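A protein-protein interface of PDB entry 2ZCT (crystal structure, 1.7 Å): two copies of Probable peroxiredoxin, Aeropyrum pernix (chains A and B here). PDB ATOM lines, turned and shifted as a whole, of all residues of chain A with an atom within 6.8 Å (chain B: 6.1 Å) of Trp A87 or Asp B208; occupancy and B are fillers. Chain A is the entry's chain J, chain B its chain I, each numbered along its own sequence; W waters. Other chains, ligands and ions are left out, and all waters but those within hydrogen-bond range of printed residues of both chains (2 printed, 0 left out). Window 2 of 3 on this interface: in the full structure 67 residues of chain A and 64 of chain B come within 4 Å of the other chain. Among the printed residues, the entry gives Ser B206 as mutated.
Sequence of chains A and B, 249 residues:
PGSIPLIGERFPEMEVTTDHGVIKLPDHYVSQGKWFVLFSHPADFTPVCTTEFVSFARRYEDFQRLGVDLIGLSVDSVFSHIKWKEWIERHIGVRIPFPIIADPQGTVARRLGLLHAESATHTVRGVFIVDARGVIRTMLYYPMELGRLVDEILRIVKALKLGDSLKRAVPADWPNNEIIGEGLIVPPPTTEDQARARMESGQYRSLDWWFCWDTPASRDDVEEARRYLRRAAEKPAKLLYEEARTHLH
OD2 of Asp B208 is in hydrogen-bond range of NE1 of Trp A87 (3.2 Å).
The backbone carbonyl oxygen (O) of Asp B208 lies within hydrogen-bond range of the side-chain hydroxyl (OG) of Ser B206, at 2.8 Å.
NE1 of Trp B210 sits at hydrogen-bond distance from OD2 of Asp B208 (2.9 Å).
The side-chain hydroxyl (OG1) of Thr A50 is in hydrogen-bond range of the indole nitrogen (NE1) of Trp A84 (2.9 Å).
The side-chain sulfur of Cys B212 sits at hydrogen-bond distance from the backbone carbonyl oxygen of Asp B208 (3.7 Å).
Trp B210 touches Phe A45.
Trp B210 touches Thr A50.
CE1 of Phe B211 touches CG2 of Thr A50, 3.9 Å away.
CZ2 of Trp A87 touches O of Leu B207 (3.6 Å).
Trp A87 touches Trp B210.
Leu B207 touches Ile A92.
Of the printed residues of chain B, Ile A92 touches Leu B207.
Printed residues of chain A within 4 Å of Leu B207: Trp A87 (3.6 Å) and Ile A92 (3.8 Å).
Printed residues of chain B within 4 Å of Phe A45: Trp B210 (3.2 Å).
Cys B212 touches none of the printed residues of chain A.
Ile A88 touches none of the printed residues of chain B.
The nearest residue of chain B that does not touch Trp A87 is Phe B211 (4.4 Å).
The nearest residue of chain A that does not touch Asp B208 is Phe A45 (5.6 Å).
The nearest printed residue of chain A that does not touch Leu B207 is His A91 (4.5 Å).
Of the 8 printed residues of chain B, 4 touch a printed residue of chain A.
Printed residues of chain B that touch a printed residue of chain A: Leu B207, Asp B208, Trp B210 and Phe B211.
Hydrophobic or aromatic side chains of chain B within 4 Å of the printed part of chain A: Leu B207, Trp B210 and Phe B211.
Along chain B the printed residues that touch a printed residue of chain A span positions 207 to 211.
Of the 15 printed residues of chain A, 4 touch a printed residue of chain B.
Hydrophobic or aromatic side chains of chain A that line the printed part of chain B: Phe A45, Trp A87 and Ile A92.
Among the printed residues, 7 pairs touch across the chains.
Among the printed residues, no Asp or Glu carboxylate lies within 4 Å of a Lys or Arg side-chain nitrogen of the other chain.
No position is printed for both chains.
Water W2 lies within hydrogen-bond range of the backbone carbonyl oxygen (O) of Leu B207 and a ring nitrogen (ND1) of His A91.
Water W1 lies within hydrogen-bond range of the backbone carbonyl oxygen of Leu B207 (2.8 Å), the indole nitrogen of Trp A87 (3.1 Å) and the side-chain carboxylate of Asp B208 (3.5 Å).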
ATOM      1  N   PHE A  45     -16.259  -3.722   5.009  1.00  0.00           N
ATOM      2  CA  PHE A  45     -15.954  -3.158   3.664  1.00  0.00           C
ATOM      3  C   PHE A  45     -14.649  -3.697   3.123  1.00  0.00           C
ATOM      4  O   PHE A  45     -13.812  -2.968   2.516  1.00  0.00           O
ATOM      5  CB  PHE A  45     -15.949  -1.607   3.692  1.00  0.00           C
ATOM      6  CG  PHE A  45     -17.298  -1.003   3.969  1.00  0.00           C
ATOM      7  CD1 PHE A  45     -17.581  -0.444   5.218  1.00  0.00           C
ATOM      8  CD2 PHE A  45     -18.276  -0.973   2.975  1.00  0.00           C
ATOM      9  CE1 PHE A  45     -18.842   0.124   5.480  1.00  0.00           C
ATOM     10  CE2 PHE A  45     -19.543  -0.397   3.221  1.00  0.00           C
ATOM     11  CZ  PHE A  45     -19.821   0.137   4.481  1.00  0.00           C
ATOM     12  N   THR A  50     -16.535  -9.943   2.102  1.00  0.00           N
ATOM     13  CA  THR A  50     -17.830  -9.696   1.435  1.00  0.00           C
ATOM     14  C   THR A  50     -18.237 -10.949   0.617  1.00  0.00           C
ATOM     15  O   THR A  50     -19.400 -11.370   0.646  1.00  0.00           O
ATOM     16  CB  THR A  50     -17.749  -8.422   0.567  1.00  0.00           C
ATOM     17  OG1 THR A  50     -17.584  -7.279   1.442  1.00  0.00           O
ATOM     18  CG2 THR A  50     -19.011  -8.233  -0.299  1.00  0.00           C
ATOM     19  N   ILE A  82     -24.066  -2.360   9.817  1.00  0.00           N
ATOM     20  CA  ILE A  82     -25.345  -2.196   9.179  1.00  0.00           C
ATOM     21  C   ILE A  82     -25.146  -1.538   7.828  1.00  0.00           C
ATOM     22  O   ILE A  82     -25.820  -1.907   6.855  1.00  0.00           O
ATOM     23  CB  ILE A  82     -26.353  -1.449  10.093  1.00  0.00           C
ATOM     24  CG1 ILE A  82     -26.587  -2.259  11.380  1.00  0.00           C
ATOM     25  CG2 ILE A  82     -27.693  -1.145   9.314  1.00  0.00           C
ATOM     26  CD1 ILE A  82     -27.365  -1.494  12.470  1.00  0.00           C
ATOM     27  N   LYS A  83     -24.245  -0.553   7.769  1.00  0.00           N
ATOM     28  CA  LYS A  83     -23.906   0.108   6.494  1.00  0.00           C
ATOM     29  C   LYS A  83     -23.303  -0.873   5.469  1.00  0.00           C
ATOM     30  O   LYS A  83     -23.661  -0.842   4.289  1.00  0.00           O
ATOM     31  CB  LYS A  83     -22.966   1.270   6.694  1.00  0.00           C
ATOM     32  CG  LYS A  83     -23.557   2.468   7.454  1.00  0.00           C
ATOM     33  CD  LYS A  83     -24.895   2.951   6.876  1.00  0.00           C
ATOM     34  CE  LYS A  83     -24.734   3.558   5.505  1.00  0.00           C
ATOM     35  NZ  LYS A  83     -26.061   3.877   4.912  1.00  0.00           N
ATOM     36  N   TRP A  84     -22.378  -1.718   5.921  1.00  0.00           N
ATOM     37  CA  TRP A  84     -21.774  -2.750   5.056  1.00  0.00           C
ATOM     38  C   TRP A  84     -22.847  -3.699   4.520  1.00  0.00           C
ATOM     39  O   TRP A  84     -22.898  -3.990   3.335  1.00  0.00           O
ATOM     40  CB  TRP A  84     -20.720  -3.491   5.859  1.00  0.00           C
ATOM     41  CG  TRP A  84     -19.900  -4.526   5.148  1.00  0.00           C
ATOM     42  CD1 TRP A  84     -19.678  -4.643   3.803  1.00  0.00           C
ATOM     43  CD2 TRP A  84     -19.086  -5.522   5.783  1.00  0.00           C
ATOM     44  NE1 TRP A  84     -18.801  -5.707   3.554  1.00  0.00           N
ATOM     45  CE2 TRP A  84     -18.433  -6.261   4.753  1.00  0.00           C
ATOM     46  CE3 TRP A  84     -18.877  -5.896   7.124  1.00  0.00           C
ATOM     47  CZ2 TRP A  84     -17.544  -7.321   5.029  1.00  0.00           C
ATOM     48  CZ3 TRP A  84     -17.993  -6.960   7.403  1.00  0.00           C
ATOM     49  CH2 TRP A  84     -17.335  -7.663   6.351  1.00  0.00           C
ATOM     50  N   LYS A  85     -23.737  -4.168   5.377  1.00  0.00           N
ATOM     51  CA  LYS A  85     -24.841  -5.009   4.920  1.00  0.00           C
ATOM     52  C   LYS A  85     -25.766  -4.332   3.913  1.00  0.00           C
ATOM     53  O   LYS A  85     -26.191  -4.933   2.918  1.00  0.00           O
ATOM     54  CB  LYS A  85     -25.659  -5.473   6.114  1.00  0.00           C
ATOM     55  CG  LYS A  85     -24.969  -6.507   6.977  1.00  0.00           C
ATOM     56  CD  LYS A  85     -25.875  -6.744   8.189  1.00  0.00           C
ATOM     57  CE  LYS A  85     -25.784  -8.166   8.628  1.00  0.00           C
ATOM     58  NZ  LYS A  85     -26.505  -8.420   9.909  1.00  0.00           N
ATOM     59  N   GLU A  86     -26.069  -3.059   4.162  1.00  0.00           N
ATOM     60  CA  GLU A  86     -26.857  -2.255   3.232  1.00  0.00           C
ATOM     61  C   GLU A  86     -26.175  -2.175   1.888  1.00  0.00           C
ATOM     62  O   GLU A  86     -26.834  -2.335   0.861  1.00  0.00           O
ATOM     63  CB  GLU A  86     -27.030  -0.825   3.772  1.00  0.00           C
ATOM     64  CG  GLU A  86     -28.137  -0.727   4.756  1.00  0.00           C
ATOM     65  CD  GLU A  86     -28.398   0.732   5.103  1.00  0.00           C
ATOM     66  OE1 GLU A  86     -27.468   1.397   5.561  1.00  0.00           O
ATOM     67  OE2 GLU A  86     -29.518   1.212   4.881  1.00  0.00           O
ATOM     68  N   TRP A  87     -24.851  -1.980   1.903  1.00  0.00           N
ATOM     69  CA  TRP A  87     -24.047  -1.911   0.680  1.00  0.00           C
ATOM     70  C   TRP A  87     -24.165  -3.234  -0.082  1.00  0.00           C
ATOM     71  O   TRP A  87     -24.402  -3.245  -1.293  1.00  0.00           O
ATOM     72  CB  TRP A  87     -22.576  -1.586   0.973  1.00  0.00           C
ATOM     73  CG  TRP A  87     -21.758  -1.431  -0.308  1.00  0.00           C
ATOM     74  CD1 TRP A  87     -21.438  -0.261  -0.956  1.00  0.00           C
ATOM     75  CD2 TRP A  87     -21.213  -2.490  -1.110  1.00  0.00           C
ATOM     76  NE1 TRP A  87     -20.703  -0.534  -2.093  1.00  0.00           N
ATOM     77  CE2 TRP A  87     -20.557  -1.890  -2.215  1.00  0.00           C
ATOM     78  CE3 TRP A  87     -21.183  -3.885  -0.984  1.00  0.00           C
ATOM     79  CZ2 TRP A  87     -19.911  -2.649  -3.210  1.00  0.00           C
ATOM     80  CZ3 TRP A  87     -20.564  -4.640  -1.981  1.00  0.00           C
ATOM     81  CH2 TRP A  87     -19.920  -4.011  -3.077  1.00  0.00           C
ATOM     82  N   ILE A  88     -24.051  -4.352   0.634  1.00  0.00           N
ATOM     83  CA  ILE A  88     -24.110  -5.674  -0.051  1.00  0.00           C
ATOM     84  C   ILE A  88     -25.469  -5.874  -0.734  1.00  0.00           C
ATOM     85  O   ILE A  88     -25.532  -6.271  -1.897  1.00  0.00           O
ATOM     86  CB  ILE A  88     -23.765  -6.859   0.902  1.00  0.00           C
ATOM     87  CG1 ILE A  88     -22.303  -6.747   1.343  1.00  0.00           C
ATOM     88  CG2 ILE A  88     -23.947  -8.230   0.170  1.00  0.00           C
ATOM     89  CD1 ILE A  88     -21.912  -7.695   2.451  1.00  0.00           C
ATOM     90  N   GLU A  89     -26.551  -5.594  -0.010  1.00  0.00           N
ATOM     91  CA  GLU A  89     -27.887  -5.795  -0.565  1.00  0.00           C
ATOM     92  C   GLU A  89     -28.137  -4.884  -1.772  1.00  0.00           C
ATOM     93  O   GLU A  89     -28.700  -5.322  -2.782  1.00  0.00           O
ATOM     94  CB  GLU A  89     -28.967  -5.612   0.490  1.00  0.00           C
ATOM     95  CG  GLU A  89     -30.371  -5.733  -0.106  1.00  0.00           C
ATOM     96  CD  GLU A  89     -31.487  -5.785   0.936  1.00  0.00           C
ATOM     97  OE1 GLU A  89     -32.671  -5.801   0.523  1.00  0.00           O
ATOM     98  OE2 GLU A  89     -31.208  -5.779   2.151  1.00  0.00           O
ATOM     99  N   ARG A  90     -27.677  -3.635  -1.680  1.00  0.00           N
ATOM    100  CA  ARG A  90     -27.784  -2.663  -2.772  1.00  0.00           C
ATOM    101  C   ARG A  90     -26.967  -3.018  -3.999  1.00  0.00           C
ATOM    102  O   ARG A  90     -27.497  -2.970  -5.106  1.00  0.00           O
ATOM    103  CB  ARG A  90     -27.434  -1.252  -2.297  1.00  0.00           C
ATOM    104  CG  ARG A  90     -27.700  -0.132  -3.328  1.00  0.00           C
ATOM    105  CD  ARG A  90     -28.333   1.145  -2.687  1.00  0.00           C
ATOM    106  NE  ARG A  90     -27.695   1.612  -1.443  1.00  0.00           N
ATOM    107  CZ  ARG A  90     -28.280   1.614  -0.234  1.00  0.00           C
ATOM    108  NH1 ARG A  90     -29.523   1.163  -0.072  1.00  0.00           N
ATOM    109  NH2 ARG A  90     -27.617   2.064   0.826  1.00  0.00           N
ATOM    110  N   HIS A  91     -25.697  -3.379  -3.809  1.00  0.00           N
ATOM    111  CA  HIS A  91     -24.775  -3.571  -4.943  1.00  0.00           C
ATOM    112  C   HIS A  91     -24.625  -4.989  -5.487  1.00  0.00           C
ATOM    113  O   HIS A  91     -24.285  -5.158  -6.653  1.00  0.00           O
ATOM    114  CB  HIS A  91     -23.410  -2.929  -4.659  1.00  0.00           C
ATOM    115  CG  HIS A  91     -23.498  -1.455  -4.440  1.00  0.00           C
ATOM    116  ND1 HIS A  91     -23.376  -0.539  -5.463  1.00  0.00           N
ATOM    117  CD2 HIS A  91     -23.773  -0.740  -3.324  1.00  0.00           C
ATOM    118  CE1 HIS A  91     -23.529   0.681  -4.975  1.00  0.00           C
ATOM    119  NE2 HIS A  91     -23.776   0.583  -3.681  1.00  0.00           N
ATOM    120  N   ILE A  92     -24.868  -5.992  -4.654  1.00  0.00           N
ATOM    121  CA  ILE A  92     -24.767  -7.397  -5.074  1.00  0.00           C
ATOM    122  C   ILE A  92     -26.168  -8.014  -5.166  1.00  0.00           C
ATOM    123  O   ILE A  92     -26.376  -9.000  -5.882  1.00  0.00           O
ATOM    124  CB  ILE A  92     -23.795  -8.198  -4.137  1.00  0.00           C
ATOM    125  CG1 ILE A  92     -22.390  -7.571  -4.211  1.00  0.00           C
ATOM    126  CG2 ILE A  92     -23.720  -9.674  -4.542  1.00  0.00           C
ATOM    127  CD1 ILE A  92     -21.406  -8.057  -3.175  1.00  0.00           C
ATOM    128  N   GLY A  93     -27.123  -7.402  -4.473  1.00  0.00           N
ATOM    129  CA  GLY A  93     -28.525  -7.813  -4.513  1.00  0.00           C
ATOM    130  C   GLY A  93     -28.837  -8.968  -3.590  1.00  0.00           C
ATOM    131  O   GLY A  93     -29.855  -9.652  -3.755  1.00  0.00           O
ATOM    132  N   VAL A  94     -27.969  -9.185  -2.604  1.00  0.00           N
ATOM    133  CA  VAL A  94     -28.121 -10.275  -1.657  1.00  0.00           C
ATOM    134  C   VAL A  94     -28.266  -9.697  -0.255  1.00  0.00           C
ATOM    135  O   VAL A  94     -27.374  -8.990   0.229  1.00  0.00           O
ATOM    136  CB  VAL A  94     -26.900 -11.259  -1.706  1.00  0.00           C
ATOM    137  CG1 VAL A  94     -27.034 -12.377  -0.621  1.00  0.00           C
ATOM    138  CG2 VAL A  94     -26.763 -11.860  -3.092  1.00  0.00           C
ATOM    139  N   MET B 199      -9.924   4.039  -8.942  1.00  0.00           N
ATOM    140  CA  MET B 199     -11.183   4.251  -9.662  1.00  0.00           C
ATOM    141  C   MET B 199     -10.996   5.075 -10.945  1.00  0.00           C
ATOM    142  O   MET B 199     -11.641   4.793 -11.969  1.00  0.00           O
ATOM    143  CB  MET B 199     -12.243   4.878  -8.753  1.00  0.00           C
ATOM    144  CG  MET B 199     -12.700   3.986  -7.608  1.00  0.00           C
ATOM    145  SD  MET B 199     -13.309   2.359  -8.158  1.00  0.00           S
ATOM    146  CE  MET B 199     -11.797   1.460  -8.380  1.00  0.00           C
ATOM    147  N   SER B 206     -14.993  -3.675 -11.172  1.00  0.00           N
ATOM    148  CA  SER B 206     -15.160  -3.095  -9.839  1.00  0.00           C
ATOM    149  C   SER B 206     -16.602  -3.023  -9.397  1.00  0.00           C
ATOM    150  O   SER B 206     -17.495  -2.770 -10.215  1.00  0.00           O
ATOM    151  CB  SER B 206     -14.548  -1.688  -9.828  1.00  0.00           C
ATOM    152  OG  SER B 206     -14.582  -1.101  -8.532  1.00  0.00           O
ATOM    153  N   LEU B 207     -16.822  -3.244  -8.099  1.00  0.00           N
ATOM    154  CA  LEU B 207     -18.101  -2.976  -7.459  1.00  0.00           C
ATOM    155  C   LEU B 207     -18.011  -1.734  -6.571  1.00  0.00           C
ATOM    156  O   LEU B 207     -19.019  -1.085  -6.311  1.00  0.00           O
ATOM    157  CB  LEU B 207     -18.565  -4.166  -6.610  1.00  0.00           C
ATOM    158  CG  LEU B 207     -19.389  -5.241  -7.330  1.00  0.00           C
ATOM    159  CD1 LEU B 207     -18.782  -5.535  -8.627  1.00  0.00           C
ATOM    160  CD2 LEU B 207     -19.535  -6.524  -6.543  1.00  0.00           C
ATOM    161  N   ASP B 208     -16.806  -1.460  -6.073  1.00  0.00           N
ATOM    162  CA  ASP B 208     -16.503  -0.238  -5.292  1.00  0.00           C
ATOM    163  C   ASP B 208     -14.991  -0.117  -5.241  1.00  0.00           C
ATOM    164  O   ASP B 208     -14.283  -0.975  -5.766  1.00  0.00           O
ATOM    165  CB  ASP B 208     -17.128  -0.309  -3.889  1.00  0.00           C
ATOM    166  CG  ASP B 208     -17.359   1.084  -3.262  1.00  0.00           C
ATOM    167  OD1 ASP B 208     -16.917   2.093  -3.852  1.00  0.00           O
ATOM    168  OD2 ASP B 208     -18.007   1.140  -2.195  1.00  0.00           O
ATOM    169  N   TRP B 209     -14.467   0.940  -4.627  1.00  0.00           N
ATOM    170  CA  TRP B 209     -13.018   1.169  -4.706  1.00  0.00           C
ATOM    171  C   TRP B 209     -12.283   0.051  -3.951  1.00  0.00           C
ATOM    172  O   TRP B 209     -11.103  -0.219  -4.215  1.00  0.00           O
ATOM    173  CB  TRP B 209     -12.643   2.560  -4.164  1.00  0.00           C
ATOM    174  CG  TRP B 209     -13.200   2.817  -2.829  1.00  0.00           C
ATOM    175  CD1 TRP B 209     -14.402   3.418  -2.552  1.00  0.00           C
ATOM    176  CD2 TRP B 209     -12.617   2.475  -1.560  1.00  0.00           C
ATOM    177  NE1 TRP B 209     -14.598   3.461  -1.196  1.00  0.00           N
ATOM    178  CE2 TRP B 209     -13.524   2.886  -0.566  1.00  0.00           C
ATOM    179  CE3 TRP B 209     -11.420   1.839  -1.172  1.00  0.00           C
ATOM    180  CZ2 TRP B 209     -13.278   2.697   0.791  1.00  0.00           C
ATOM    181  CZ3 TRP B 209     -11.169   1.665   0.196  1.00  0.00           C
ATOM    182  CH2 TRP B 209     -12.100   2.100   1.152  1.00  0.00           C
ATOM    183  N   TRP B 210     -12.995  -0.585  -3.011  1.00  0.00           N
ATOM    184  CA  TRP B 210     -12.399  -1.604  -2.128  1.00  0.00           C
ATOM    185  C   TRP B 210     -12.684  -3.005  -2.665  1.00  0.00           C
ATOM    186  O   TRP B 210     -12.271  -3.996  -2.065  1.00  0.00           O
ATOM    187  CB  TRP B 210     -12.936  -1.498  -0.694  1.00  0.00           C
ATOM    188  CG  TRP B 210     -14.425  -1.484  -0.613  1.00  0.00           C
ATOM    189  CD1 TRP B 210     -15.257  -0.375  -0.683  1.00  0.00           C
ATOM    190  CD2 TRP B 210     -15.290  -2.619  -0.392  1.00  0.00           C
ATOM    191  NE1 TRP B 210     -16.558  -0.763  -0.541  1.00  0.00           N
ATOM    192  CE2 TRP B 210     -16.619  -2.131  -0.397  1.00  0.00           C
ATOM    193  CE3 TRP B 210     -15.065  -4.005  -0.245  1.00  0.00           C
ATOM    194  CZ2 TRP B 210     -17.740  -2.979  -0.214  1.00  0.00           C
ATOM    195  CZ3 TRP B 210     -16.177  -4.859  -0.053  1.00  0.00           C
ATOM    196  CH2 TRP B 210     -17.497  -4.337  -0.041  1.00  0.00           C
ATOM    197  N   PHE B 211     -13.382  -3.075  -3.798  1.00  0.00           N
ATOM    198  CA  PHE B 211     -13.750  -4.378  -4.375  1.00  0.00           C
ATOM    199  C   PHE B 211     -13.530  -4.327  -5.881  1.00  0.00           C
ATOM    200  O   PHE B 211     -14.462  -4.070  -6.641  1.00  0.00           O
ATOM    201  CB  PHE B 211     -15.218  -4.721  -4.031  1.00  0.00           C
ATOM    202  CG  PHE B 211     -15.590  -6.177  -4.243  1.00  0.00           C
ATOM    203  CD1 PHE B 211     -16.528  -6.780  -3.418  1.00  0.00           C
ATOM    204  CD2 PHE B 211     -14.996  -6.954  -5.233  1.00  0.00           C
ATOM    205  CE1 PHE B 211     -16.891  -8.131  -3.593  1.00  0.00           C
ATOM    206  CE2 PHE B 211     -15.361  -8.323  -5.408  1.00  0.00           C
ATOM    207  CZ  PHE B 211     -16.312  -8.892  -4.576  1.00  0.00           C
ATOM    208  N   CYS B 212     -12.266  -4.504  -6.260  1.00  0.00           N
ATOM    209  CA  CYS B 212     -11.845  -4.584  -7.656  1.00  0.00           C
ATOM    210  C   CYS B 212     -11.273  -5.970  -7.858  1.00  0.00           C
ATOM    211  O   CYS B 212     -10.723  -6.584  -6.932  1.00  0.00           O
ATOM    212  CB  CYS B 212     -10.766  -3.531  -7.967  1.00  0.00           C
ATOM    213  SG  CYS B 212     -11.390  -1.806  -7.880  1.00  0.00           S
HETATM  214  O   HOH W   1     -20.275   0.962  -4.822  1.00  0.00           O
HETATM  215  O   HOH W   2     -21.319  -1.740  -7.535  1.00  0.00           O
